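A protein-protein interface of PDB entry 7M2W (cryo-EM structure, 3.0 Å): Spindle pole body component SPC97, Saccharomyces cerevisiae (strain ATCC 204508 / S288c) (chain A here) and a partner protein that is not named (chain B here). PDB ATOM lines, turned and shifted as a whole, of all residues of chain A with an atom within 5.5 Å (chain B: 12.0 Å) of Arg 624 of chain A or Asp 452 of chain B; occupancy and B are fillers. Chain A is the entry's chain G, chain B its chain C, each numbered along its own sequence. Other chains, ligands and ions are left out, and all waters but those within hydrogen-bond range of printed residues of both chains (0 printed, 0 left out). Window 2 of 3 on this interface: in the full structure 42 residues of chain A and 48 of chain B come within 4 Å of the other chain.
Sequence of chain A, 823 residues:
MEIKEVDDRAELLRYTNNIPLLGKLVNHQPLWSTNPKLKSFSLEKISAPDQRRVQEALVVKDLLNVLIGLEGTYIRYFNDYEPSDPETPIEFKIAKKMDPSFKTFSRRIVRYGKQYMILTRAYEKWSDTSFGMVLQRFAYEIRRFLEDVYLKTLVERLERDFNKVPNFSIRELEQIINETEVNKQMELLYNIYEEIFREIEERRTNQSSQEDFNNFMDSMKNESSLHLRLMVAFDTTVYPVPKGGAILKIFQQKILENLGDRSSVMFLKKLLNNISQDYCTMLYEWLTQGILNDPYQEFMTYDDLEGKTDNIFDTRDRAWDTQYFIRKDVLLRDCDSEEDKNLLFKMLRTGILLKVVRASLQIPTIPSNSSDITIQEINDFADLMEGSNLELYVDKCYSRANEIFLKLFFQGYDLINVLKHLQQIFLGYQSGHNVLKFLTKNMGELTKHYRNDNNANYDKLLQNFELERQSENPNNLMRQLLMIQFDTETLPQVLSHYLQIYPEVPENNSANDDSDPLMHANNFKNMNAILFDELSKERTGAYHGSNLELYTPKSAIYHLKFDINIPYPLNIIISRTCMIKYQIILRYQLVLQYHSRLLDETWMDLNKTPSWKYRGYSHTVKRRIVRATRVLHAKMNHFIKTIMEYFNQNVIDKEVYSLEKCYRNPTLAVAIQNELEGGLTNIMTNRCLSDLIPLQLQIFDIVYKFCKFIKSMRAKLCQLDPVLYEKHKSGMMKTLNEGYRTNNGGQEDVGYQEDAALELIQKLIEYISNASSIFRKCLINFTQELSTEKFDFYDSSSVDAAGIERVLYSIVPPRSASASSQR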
ATOM      1  N   THR A 620     -21.814  26.404  12.961  1.00  0.00           N
ATOM      2  CA  THR A 620     -20.597  27.195  12.839  1.00  0.00           C
ATOM      3  C   THR A 620     -19.786  27.092  14.122  1.00  0.00           C
ATOM      4  O   THR A 620     -18.578  26.836  14.086  1.00  0.00           O
ATOM      5  CB  THR A 620     -20.922  28.658  12.533  1.00  0.00           C
ATOM      6  OG1 THR A 620     -21.923  28.725  11.509  1.00  0.00           O
ATOM      7  CG2 THR A 620     -19.674  29.396  12.075  1.00  0.00           C
ATOM      8  N   VAL A 621     -20.453  27.297  15.259  1.00  0.00           N
ATOM      9  CA  VAL A 621     -19.801  27.126  16.552  1.00  0.00           C
ATOM     10  C   VAL A 621     -19.269  25.707  16.691  1.00  0.00           C
ATOM     11  O   VAL A 621     -18.176  25.490  17.230  1.00  0.00           O
ATOM     12  CB  VAL A 621     -20.774  27.488  17.690  1.00  0.00           C
ATOM     13  CG1 VAL A 621     -20.314  26.891  19.014  1.00  0.00           C
ATOM     14  CG2 VAL A 621     -20.924  28.995  17.797  1.00  0.00           C
ATOM     15  N   LYS A 622     -20.025  24.722  16.192  1.00  0.00           N
ATOM     16  CA  LYS A 622     -19.576  23.337  16.258  1.00  0.00           C
ATOM     17  C   LYS A 622     -18.194  23.167  15.658  1.00  0.00           C
ATOM     18  O   LYS A 622     -17.318  22.609  16.319  1.00  0.00           O
ATOM     19  CB  LYS A 622     -20.586  22.402  15.577  1.00  0.00           C
ATOM     20  CG  LYS A 622     -20.668  22.491  14.061  1.00  0.00           C
ATOM     21  CD  LYS A 622     -21.299  21.240  13.474  1.00  0.00           C
ATOM     22  CE  LYS A 622     -21.217  21.245  11.957  1.00  0.00           C
ATOM     23  NZ  LYS A 622     -21.812  20.017  11.365  1.00  0.00           N
ATOM     24  N   ARG A 623     -17.940  23.730  14.480  1.00  0.00           N
ATOM     25  CA  ARG A 623     -16.616  23.608  13.895  1.00  0.00           C
ATOM     26  C   ARG A 623     -15.594  24.371  14.732  1.00  0.00           C
ATOM     27  O   ARG A 623     -14.802  23.747  15.445  1.00  0.00           O
ATOM     28  CB  ARG A 623     -16.645  24.106  12.447  1.00  0.00           C
ATOM     29  CG  ARG A 623     -17.799  23.521  11.654  1.00  0.00           C
ATOM     30  CD  ARG A 623     -17.779  23.967  10.209  1.00  0.00           C
ATOM     31  NE  ARG A 623     -17.816  25.420  10.077  1.00  0.00           N
ATOM     32  CZ  ARG A 623     -18.868  26.104   9.641  1.00  0.00           C
ATOM     33  NH1 ARG A 623     -19.979  25.468   9.292  1.00  0.00           N
ATOM     34  NH2 ARG A 623     -18.812  27.426   9.552  1.00  0.00           N
ATOM     35  N   ARG A 624     -15.733  25.700  14.791  1.00  0.00           N
ATOM     36  CA  ARG A 624     -14.687  26.558  15.336  1.00  0.00           C
ATOM     37  C   ARG A 624     -14.406  26.287  16.807  1.00  0.00           C
ATOM     38  O   ARG A 624     -13.393  26.761  17.333  1.00  0.00           O
ATOM     39  CB  ARG A 624     -15.062  28.026  15.148  1.00  0.00           C
ATOM     40  CG  ARG A 624     -15.383  28.406  13.717  1.00  0.00           C
ATOM     41  CD  ARG A 624     -14.132  28.374  12.862  1.00  0.00           C
ATOM     42  NE  ARG A 624     -13.019  29.055  13.516  1.00  0.00           N
ATOM     43  CZ  ARG A 624     -12.834  30.370  13.502  1.00  0.00           C
ATOM     44  NH1 ARG A 624     -13.687  31.156  12.862  1.00  0.00           N
ATOM     45  NH2 ARG A 624     -11.790  30.898  14.124  1.00  0.00           N
ATOM     46  N   ILE A 625     -15.272  25.546  17.494  1.00  0.00           N
ATOM     47  CA  ILE A 625     -15.026  25.148  18.874  1.00  0.00           C
ATOM     48  C   ILE A 625     -14.734  23.657  18.974  1.00  0.00           C
ATOM     49  O   ILE A 625     -13.597  23.256  19.226  1.00  0.00           O
ATOM     50  CB  ILE A 625     -16.206  25.548  19.788  1.00  0.00           C
ATOM     51  CG1 ILE A 625     -16.295  27.069  19.905  1.00  0.00           C
ATOM     52  CG2 ILE A 625     -16.056  24.922  21.164  1.00  0.00           C
ATOM     53  CD1 ILE A 625     -14.961  27.725  20.155  1.00  0.00           C
ATOM     54  N   VAL A 626     -15.726  22.815  18.691  1.00  0.00           N
ATOM     55  CA  VAL A 626     -15.591  21.398  18.985  1.00  0.00           C
ATOM     56  C   VAL A 626     -14.686  20.723  17.965  1.00  0.00           C
ATOM     57  O   VAL A 626     -13.862  19.877  18.322  1.00  0.00           O
ATOM     58  CB  VAL A 626     -16.981  20.739  19.042  1.00  0.00           C
ATOM     59  CG1 VAL A 626     -16.858  19.233  19.128  1.00  0.00           C
ATOM     60  CG2 VAL A 626     -17.769  21.281  20.223  1.00  0.00           C
ATOM     61  N   ARG A 627     -14.812  21.077  16.683  1.00  0.00           N
ATOM     62  CA  ARG A 627     -14.010  20.389  15.682  1.00  0.00           C
ATOM     63  C   ARG A 627     -12.549  20.799  15.788  1.00  0.00           C
ATOM     64  O   ARG A 627     -11.655  19.950  15.702  1.00  0.00           O
ATOM     65  CB  ARG A 627     -14.553  20.671  14.284  1.00  0.00           C
ATOM     66  CG  ARG A 627     -13.866  19.889  13.184  1.00  0.00           C
ATOM     67  CD  ARG A 627     -14.800  19.693  12.007  1.00  0.00           C
ATOM     68  NE  ARG A 627     -15.849  18.727  12.311  1.00  0.00           N
ATOM     69  CZ  ARG A 627     -16.945  18.561  11.579  1.00  0.00           C
ATOM     70  NH1 ARG A 627     -17.141  19.302  10.497  1.00  0.00           N
ATOM     71  NH2 ARG A 627     -17.848  17.657  11.930  1.00  0.00           N
ATOM     72  N   ALA A 628     -12.289  22.093  15.987  1.00  0.00           N
ATOM     73  CA  ALA A 628     -10.921  22.540  16.225  1.00  0.00           C
ATOM     74  C   ALA A 628     -10.354  21.920  17.495  1.00  0.00           C
ATOM     75  O   ALA A 628      -9.182  21.526  17.530  1.00  0.00           O
ATOM     76  CB  ALA A 628     -10.869  24.064  16.299  1.00  0.00           C
ATOM     77  N   LEU A 764     -13.727  31.481  23.460  1.00  0.00           N
ATOM     78  CA  LEU A 764     -13.240  30.125  23.231  1.00  0.00           C
ATOM     79  C   LEU A 764     -12.638  29.979  21.840  1.00  0.00           C
ATOM     80  O   LEU A 764     -11.621  29.298  21.676  1.00  0.00           O
ATOM     81  CB  LEU A 764     -14.357  29.101  23.442  1.00  0.00           C
ATOM     82  CG  LEU A 764     -15.129  29.127  24.761  1.00  0.00           C
ATOM     83  CD1 LEU A 764     -16.060  27.928  24.861  1.00  0.00           C
ATOM     84  CD2 LEU A 764     -14.173  29.172  25.941  1.00  0.00           C
ATOM     85  N   ILE A 765     -13.245  30.602  20.827  1.00  0.00           N
ATOM     86  CA  ILE A 765     -12.646  30.587  19.491  1.00  0.00           C
ATOM     87  C   ILE A 765     -11.240  31.171  19.534  1.00  0.00           C
ATOM     88  O   ILE A 765     -10.290  30.598  18.984  1.00  0.00           O
ATOM     89  CB  ILE A 765     -13.529  31.339  18.478  1.00  0.00           C
ATOM     90  CG1 ILE A 765     -14.969  30.834  18.508  1.00  0.00           C
ATOM     91  CG2 ILE A 765     -12.949  31.221  17.084  1.00  0.00           C
ATOM     92  CD1 ILE A 765     -15.957  31.755  17.826  1.00  0.00           C
ATOM     93  N   ILE A 768      -8.786  28.899  21.430  1.00  0.00           N
ATOM     94  CA  ILE A 768      -8.497  27.668  20.706  1.00  0.00           C
ATOM     95  C   ILE A 768      -7.566  27.952  19.536  1.00  0.00           C
ATOM     96  O   ILE A 768      -6.643  27.176  19.256  1.00  0.00           O
ATOM     97  CB  ILE A 768      -9.811  27.004  20.253  1.00  0.00           C
ATOM     98  CG1 ILE A 768     -10.476  26.299  21.434  1.00  0.00           C
ATOM     99  CG2 ILE A 768      -9.560  26.020  19.126  1.00  0.00           C
ATOM    100  CD1 ILE A 768     -11.851  25.770  21.126  1.00  0.00           C
ATOM    101  N   SER A 769      -7.774  29.080  18.850  1.00  0.00           N
ATOM    102  CA  SER A 769      -6.831  29.473  17.808  1.00  0.00           C
ATOM    103  C   SER A 769      -5.459  29.771  18.399  1.00  0.00           C
ATOM    104  O   SER A 769      -4.432  29.458  17.788  1.00  0.00           O
ATOM    105  CB  SER A 769      -7.361  30.684  17.043  1.00  0.00           C
ATOM    106  OG  SER A 769      -6.708  30.818  15.793  1.00  0.00           O
ATOM    107  N   GLU B 264     -18.024  10.365  16.049  1.00  0.00           N
ATOM    108  CA  GLU B 264     -18.757  10.114  14.815  1.00  0.00           C
ATOM    109  C   GLU B 264     -18.013   9.193  13.864  1.00  0.00           C
ATOM    110  O   GLU B 264     -18.640   8.632  12.960  1.00  0.00           O
ATOM    111  CB  GLU B 264     -19.073  11.428  14.087  1.00  0.00           C
ATOM    112  CG  GLU B 264     -19.899  12.416  14.895  1.00  0.00           C
ATOM    113  CD  GLU B 264     -19.051  13.484  15.561  1.00  0.00           C
ATOM    114  OE1 GLU B 264     -19.380  14.681  15.421  1.00  0.00           O
ATOM    115  OE2 GLU B 264     -18.055  13.125  16.222  1.00  0.00           O
ATOM    116  N   ASP B 443     -10.701  17.521   2.055  1.00  0.00           N
ATOM    117  CA  ASP B 443      -9.882  18.560   2.671  1.00  0.00           C
ATOM    118  C   ASP B 443     -10.740  19.658   3.285  1.00  0.00           C
ATOM    119  O   ASP B 443     -10.300  20.342   4.216  1.00  0.00           O
ATOM    120  CB  ASP B 443      -8.912  19.145   1.644  1.00  0.00           C
ATOM    121  CG  ASP B 443      -9.597  20.036   0.624  1.00  0.00           C
ATOM    122  OD1 ASP B 443     -10.803  19.840   0.362  1.00  0.00           O
ATOM    123  OD2 ASP B 443      -8.925  20.939   0.082  1.00  0.00           O
ATOM    124  N   SER B 444     -11.961  19.842   2.778  1.00  0.00           N
ATOM    125  CA  SER B 444     -12.858  20.866   3.298  1.00  0.00           C
ATOM    126  C   SER B 444     -13.353  20.563   4.704  1.00  0.00           C
ATOM    127  O   SER B 444     -14.138  21.348   5.245  1.00  0.00           O
ATOM    128  CB  SER B 444     -14.053  21.037   2.358  1.00  0.00           C
ATOM    129  OG  SER B 444     -15.154  21.617   3.036  1.00  0.00           O
ATOM    130  N   TYR B 445     -12.923  19.451   5.305  1.00  0.00           N
ATOM    131  CA  TYR B 445     -13.333  19.143   6.669  1.00  0.00           C
ATOM    132  C   TYR B 445     -12.809  20.182   7.651  1.00  0.00           C
ATOM    133  O   TYR B 445     -13.443  20.451   8.678  1.00  0.00           O
ATOM    134  CB  TYR B 445     -12.850  17.747   7.061  1.00  0.00           C
ATOM    135  CG  TYR B 445     -13.453  17.232   8.348  1.00  0.00           C
ATOM    136  CD1 TYR B 445     -14.793  16.875   8.414  1.00  0.00           C
ATOM    137  CD2 TYR B 445     -12.684  17.105   9.496  1.00  0.00           C
ATOM    138  CE1 TYR B 445     -15.348  16.403   9.586  1.00  0.00           C
ATOM    139  CE2 TYR B 445     -13.230  16.637  10.674  1.00  0.00           C
ATOM    140  CZ  TYR B 445     -14.563  16.286  10.713  1.00  0.00           C
ATOM    141  OH  TYR B 445     -15.114  15.819  11.883  1.00  0.00           O
ATOM    142  N   LEU B 446     -11.656  20.778   7.353  1.00  0.00           N
ATOM    143  CA  LEU B 446     -11.017  21.732   8.246  1.00  0.00           C
ATOM    144  C   LEU B 446     -10.911  23.128   7.650  1.00  0.00           C
ATOM    145  O   LEU B 446     -10.345  24.019   8.292  1.00  0.00           O
ATOM    146  CB  LEU B 446      -9.631  21.228   8.646  1.00  0.00           C
ATOM    147  CG  LEU B 446      -9.612  20.120   9.699  1.00  0.00           C
ATOM    148  CD1 LEU B 446      -8.249  20.034  10.360  1.00  0.00           C
ATOM    149  CD2 LEU B 446     -10.698  20.355  10.735  1.00  0.00           C
ATOM    150  N   ASP B 447     -11.444  23.342   6.443  1.00  0.00           N
ATOM    151  CA  ASP B 447     -11.463  24.686   5.876  1.00  0.00           C
ATOM    152  C   ASP B 447     -12.199  25.663   6.781  1.00  0.00           C
ATOM    153  O   ASP B 447     -11.588  26.595   7.315  1.00  0.00           O
ATOM    154  CB  ASP B 447     -12.107  24.666   4.489  1.00  0.00           C
ATOM    155  CG  ASP B 447     -11.101  24.432   3.381  1.00  0.00           C
ATOM    156  OD1 ASP B 447     -10.003  25.025   3.439  1.00  0.00           O
ATOM    157  OD2 ASP B 447     -11.409  23.661   2.449  1.00  0.00           O
ATOM    158  N   ASP B 448     -13.495  25.442   6.998  1.00  0.00           N
ATOM    159  CA  ASP B 448     -14.317  26.283   7.855  1.00  0.00           C
ATOM    160  C   ASP B 448     -14.018  26.078   9.336  1.00  0.00           C
ATOM    161  O   ASP B 448     -14.788  26.535  10.188  1.00  0.00           O
ATOM    162  CB  ASP B 448     -15.796  26.024   7.565  1.00  0.00           C
ATOM    163  CG  ASP B 448     -16.100  24.552   7.371  1.00  0.00           C
ATOM    164  OD1 ASP B 448     -15.192  23.722   7.588  1.00  0.00           O
ATOM    165  OD2 ASP B 448     -17.246  24.223   6.999  1.00  0.00           O
ATOM    166  N   VAL B 449     -12.919  25.400   9.658  1.00  0.00           N
ATOM    167  CA  VAL B 449     -12.500  25.165  11.036  1.00  0.00           C
ATOM    168  C   VAL B 449     -11.245  25.965  11.373  1.00  0.00           C
ATOM    169  O   VAL B 449     -11.202  26.674  12.380  1.00  0.00           O
ATOM    170  CB  VAL B 449     -12.291  23.659  11.305  1.00  0.00           C
ATOM    171  CG1 VAL B 449     -12.030  23.415  12.781  1.00  0.00           C
ATOM    172  CG2 VAL B 449     -13.498  22.868  10.836  1.00  0.00           C
ATOM    173  N   LEU B 450     -10.210  25.864  10.540  1.00  0.00           N
ATOM    174  CA  LEU B 450      -8.967  26.585  10.778  1.00  0.00           C
ATOM    175  C   LEU B 450      -8.673  27.668   9.750  1.00  0.00           C
ATOM    176  O   LEU B 450      -8.051  28.672  10.101  1.00  0.00           O
ATOM    177  CB  LEU B 450      -7.782  25.607  10.841  1.00  0.00           C
ATOM    178  CG  LEU B 450      -7.374  24.754   9.636  1.00  0.00           C
ATOM    179  CD1 LEU B 450      -6.370  25.481   8.749  1.00  0.00           C
ATOM    180  CD2 LEU B 450      -6.812  23.417  10.096  1.00  0.00           C
ATOM    181  N   VAL B 451      -9.099  27.498   8.497  1.00  0.00           N
ATOM    182  CA  VAL B 451      -8.852  28.523   7.490  1.00  0.00           C
ATOM    183  C   VAL B 451      -9.759  29.727   7.716  1.00  0.00           C
ATOM    184  O   VAL B 451      -9.303  30.876   7.707  1.00  0.00           O
ATOM    185  CB  VAL B 451      -9.031  27.942   6.076  1.00  0.00           C
ATOM    186  CG1 VAL B 451      -8.499  28.912   5.033  1.00  0.00           C
ATOM    187  CG2 VAL B 451      -8.331  26.599   5.959  1.00  0.00           C
ATOM    188  N   ASP B 452     -11.053  29.484   7.927  1.00  0.00           N
ATOM    189  CA  ASP B 452     -12.005  30.553   8.233  1.00  0.00           C
ATOM    190  C   ASP B 452     -11.848  30.951   9.701  1.00  0.00           C
ATOM    191  O   ASP B 452     -12.715  30.726  10.547  1.00  0.00           O
ATOM    192  CB  ASP B 452     -13.428  30.111   7.920  1.00  0.00           C
ATOM    193  CG  ASP B 452     -14.384  31.279   7.781  1.00  0.00           C
ATOM    194  OD1 ASP B 452     -14.571  31.766   6.646  1.00  0.00           O
ATOM    195  OD2 ASP B 452     -14.950  31.711   8.808  1.00  0.00           O
ATOM    196  N   ASP B 453     -10.705  31.566   9.991  1.00  0.00           N
ATOM    197  CA  ASP B 453     -10.353  31.929  11.359  1.00  0.00           C
ATOM    198  C   ASP B 453     -10.245  33.443  11.513  1.00  0.00           C
ATOM    199  O   ASP B 453     -10.835  34.028  12.420  1.00  0.00           O
ATOM    200  CB  ASP B 453      -9.036  31.259  11.761  1.00  0.00           C
ATOM    201  CG  ASP B 453      -8.777  31.320  13.254  1.00  0.00           C
ATOM    202  OD1 ASP B 453      -9.635  31.846  13.992  1.00  0.00           O
ATOM    203  OD2 ASP B 453      -7.712  30.837  13.691  1.00  0.00           O
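Among the printed residues, pairs that only touch across the chains: Arg 624 of chain A with Asp 448 of chain B (3.3 Å), Ala 628 of chain A with Val 449 of chain B (3.5 Å), Arg 627 of chain A with Val 449 of chain B (3.6 Å) and Arg 623 of chain A with Val 449 of chain B (3.7 Å).
The backbone NH (N) of Asp 452 of chain B sits at hydrogen-bond distance from the backbone carbonyl oxygen (O) of Asp 447 of chain B (3.0 Å).
The backbone carbonyl oxygen (O) of Lys 622 of chain A lies within hydrogen-bond range of the backbone NH (N) of Arg 627 of chain A, at 3.0 Å.
The backbone carbonyl oxygen of Arg 623 of chain A sits at hydrogen-bond distance from the backbone NH of Ala 628 of chain A, at 3.1 Å.
NE of Arg 627 of chain A is in hydrogen-bond range of OH of Tyr 445 of chain B, at 3.0 Å.
OD2 of Asp 448 of chain B is in salt-bridge range of NE of Arg 623 of chain A (3.4 Å).
The backbone carbonyl oxygen (O) of Val 449 of chain B sits at hydrogen-bond distance from the guanidinium group (NE) of Arg 624 of chain A, 3.2 Å away.
The backbone carbonyl oxygen of Asp 452 of chain B is in hydrogen-bond range of the guanidinium group of Arg 624 of chain A, at 2.5 Å.
The guanidinium group (NH2) of Arg 624 of chain A lies close to the side-chain carboxylate (OD1) of Asp 453 of chain B, at 2.4 Å.
OD2 of Asp 453 of chain B sits close to OG of Ser 769 of chain A.
Of the printed residues of chain B, Arg 624 of chain A touches Asp 448, Val 449, Asp 452 and Asp 453.
Asp 452 of chain B touches one residue of chain A.
No residue of chain B comes within 4 Å of Val 621 of chain A.
Of chain B, only Asp 448 (3.2 Å) and Val 449 (3.7 Å) come within 4 Å of Arg 623 of chain A.
No residue of chain B comes within 4 Å of Val 626 of chain A.
No residue of chain B comes within 4 Å of Ile 765 of chain A.
No residue of chain B comes within 4 Å of Ile 768 of chain A.
Of the printed residues of chain A, Tyr 445 of chain B touches Arg 627.
Of the printed residues of chain A, Asp 453 of chain B touches Arg 624 (2.4 Å) and Ser 769 (2.3 Å).
Printed residues of chain A within 4 Å of Asp 448 of chain B: Arg 623 and Arg 624.
Printed residues of chain A within 4 Å of Val 449 of chain B: Arg 623 (3.7 Å), Arg 624 (3.2 Å), Arg 627 (3.6 Å) and Ala 628 (3.5 Å).
Printed residues of chain B within 4 Å of Ser 769 of chain A: Asp 453.
The nearest residue of chain B that does not touch Arg 624 of chain A is Leu 450 of chain B (5.2 Å).
The nearest printed residue of chain B that does not touch Arg 627 of chain A is Leu 446 of chain B (4.03 Å).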
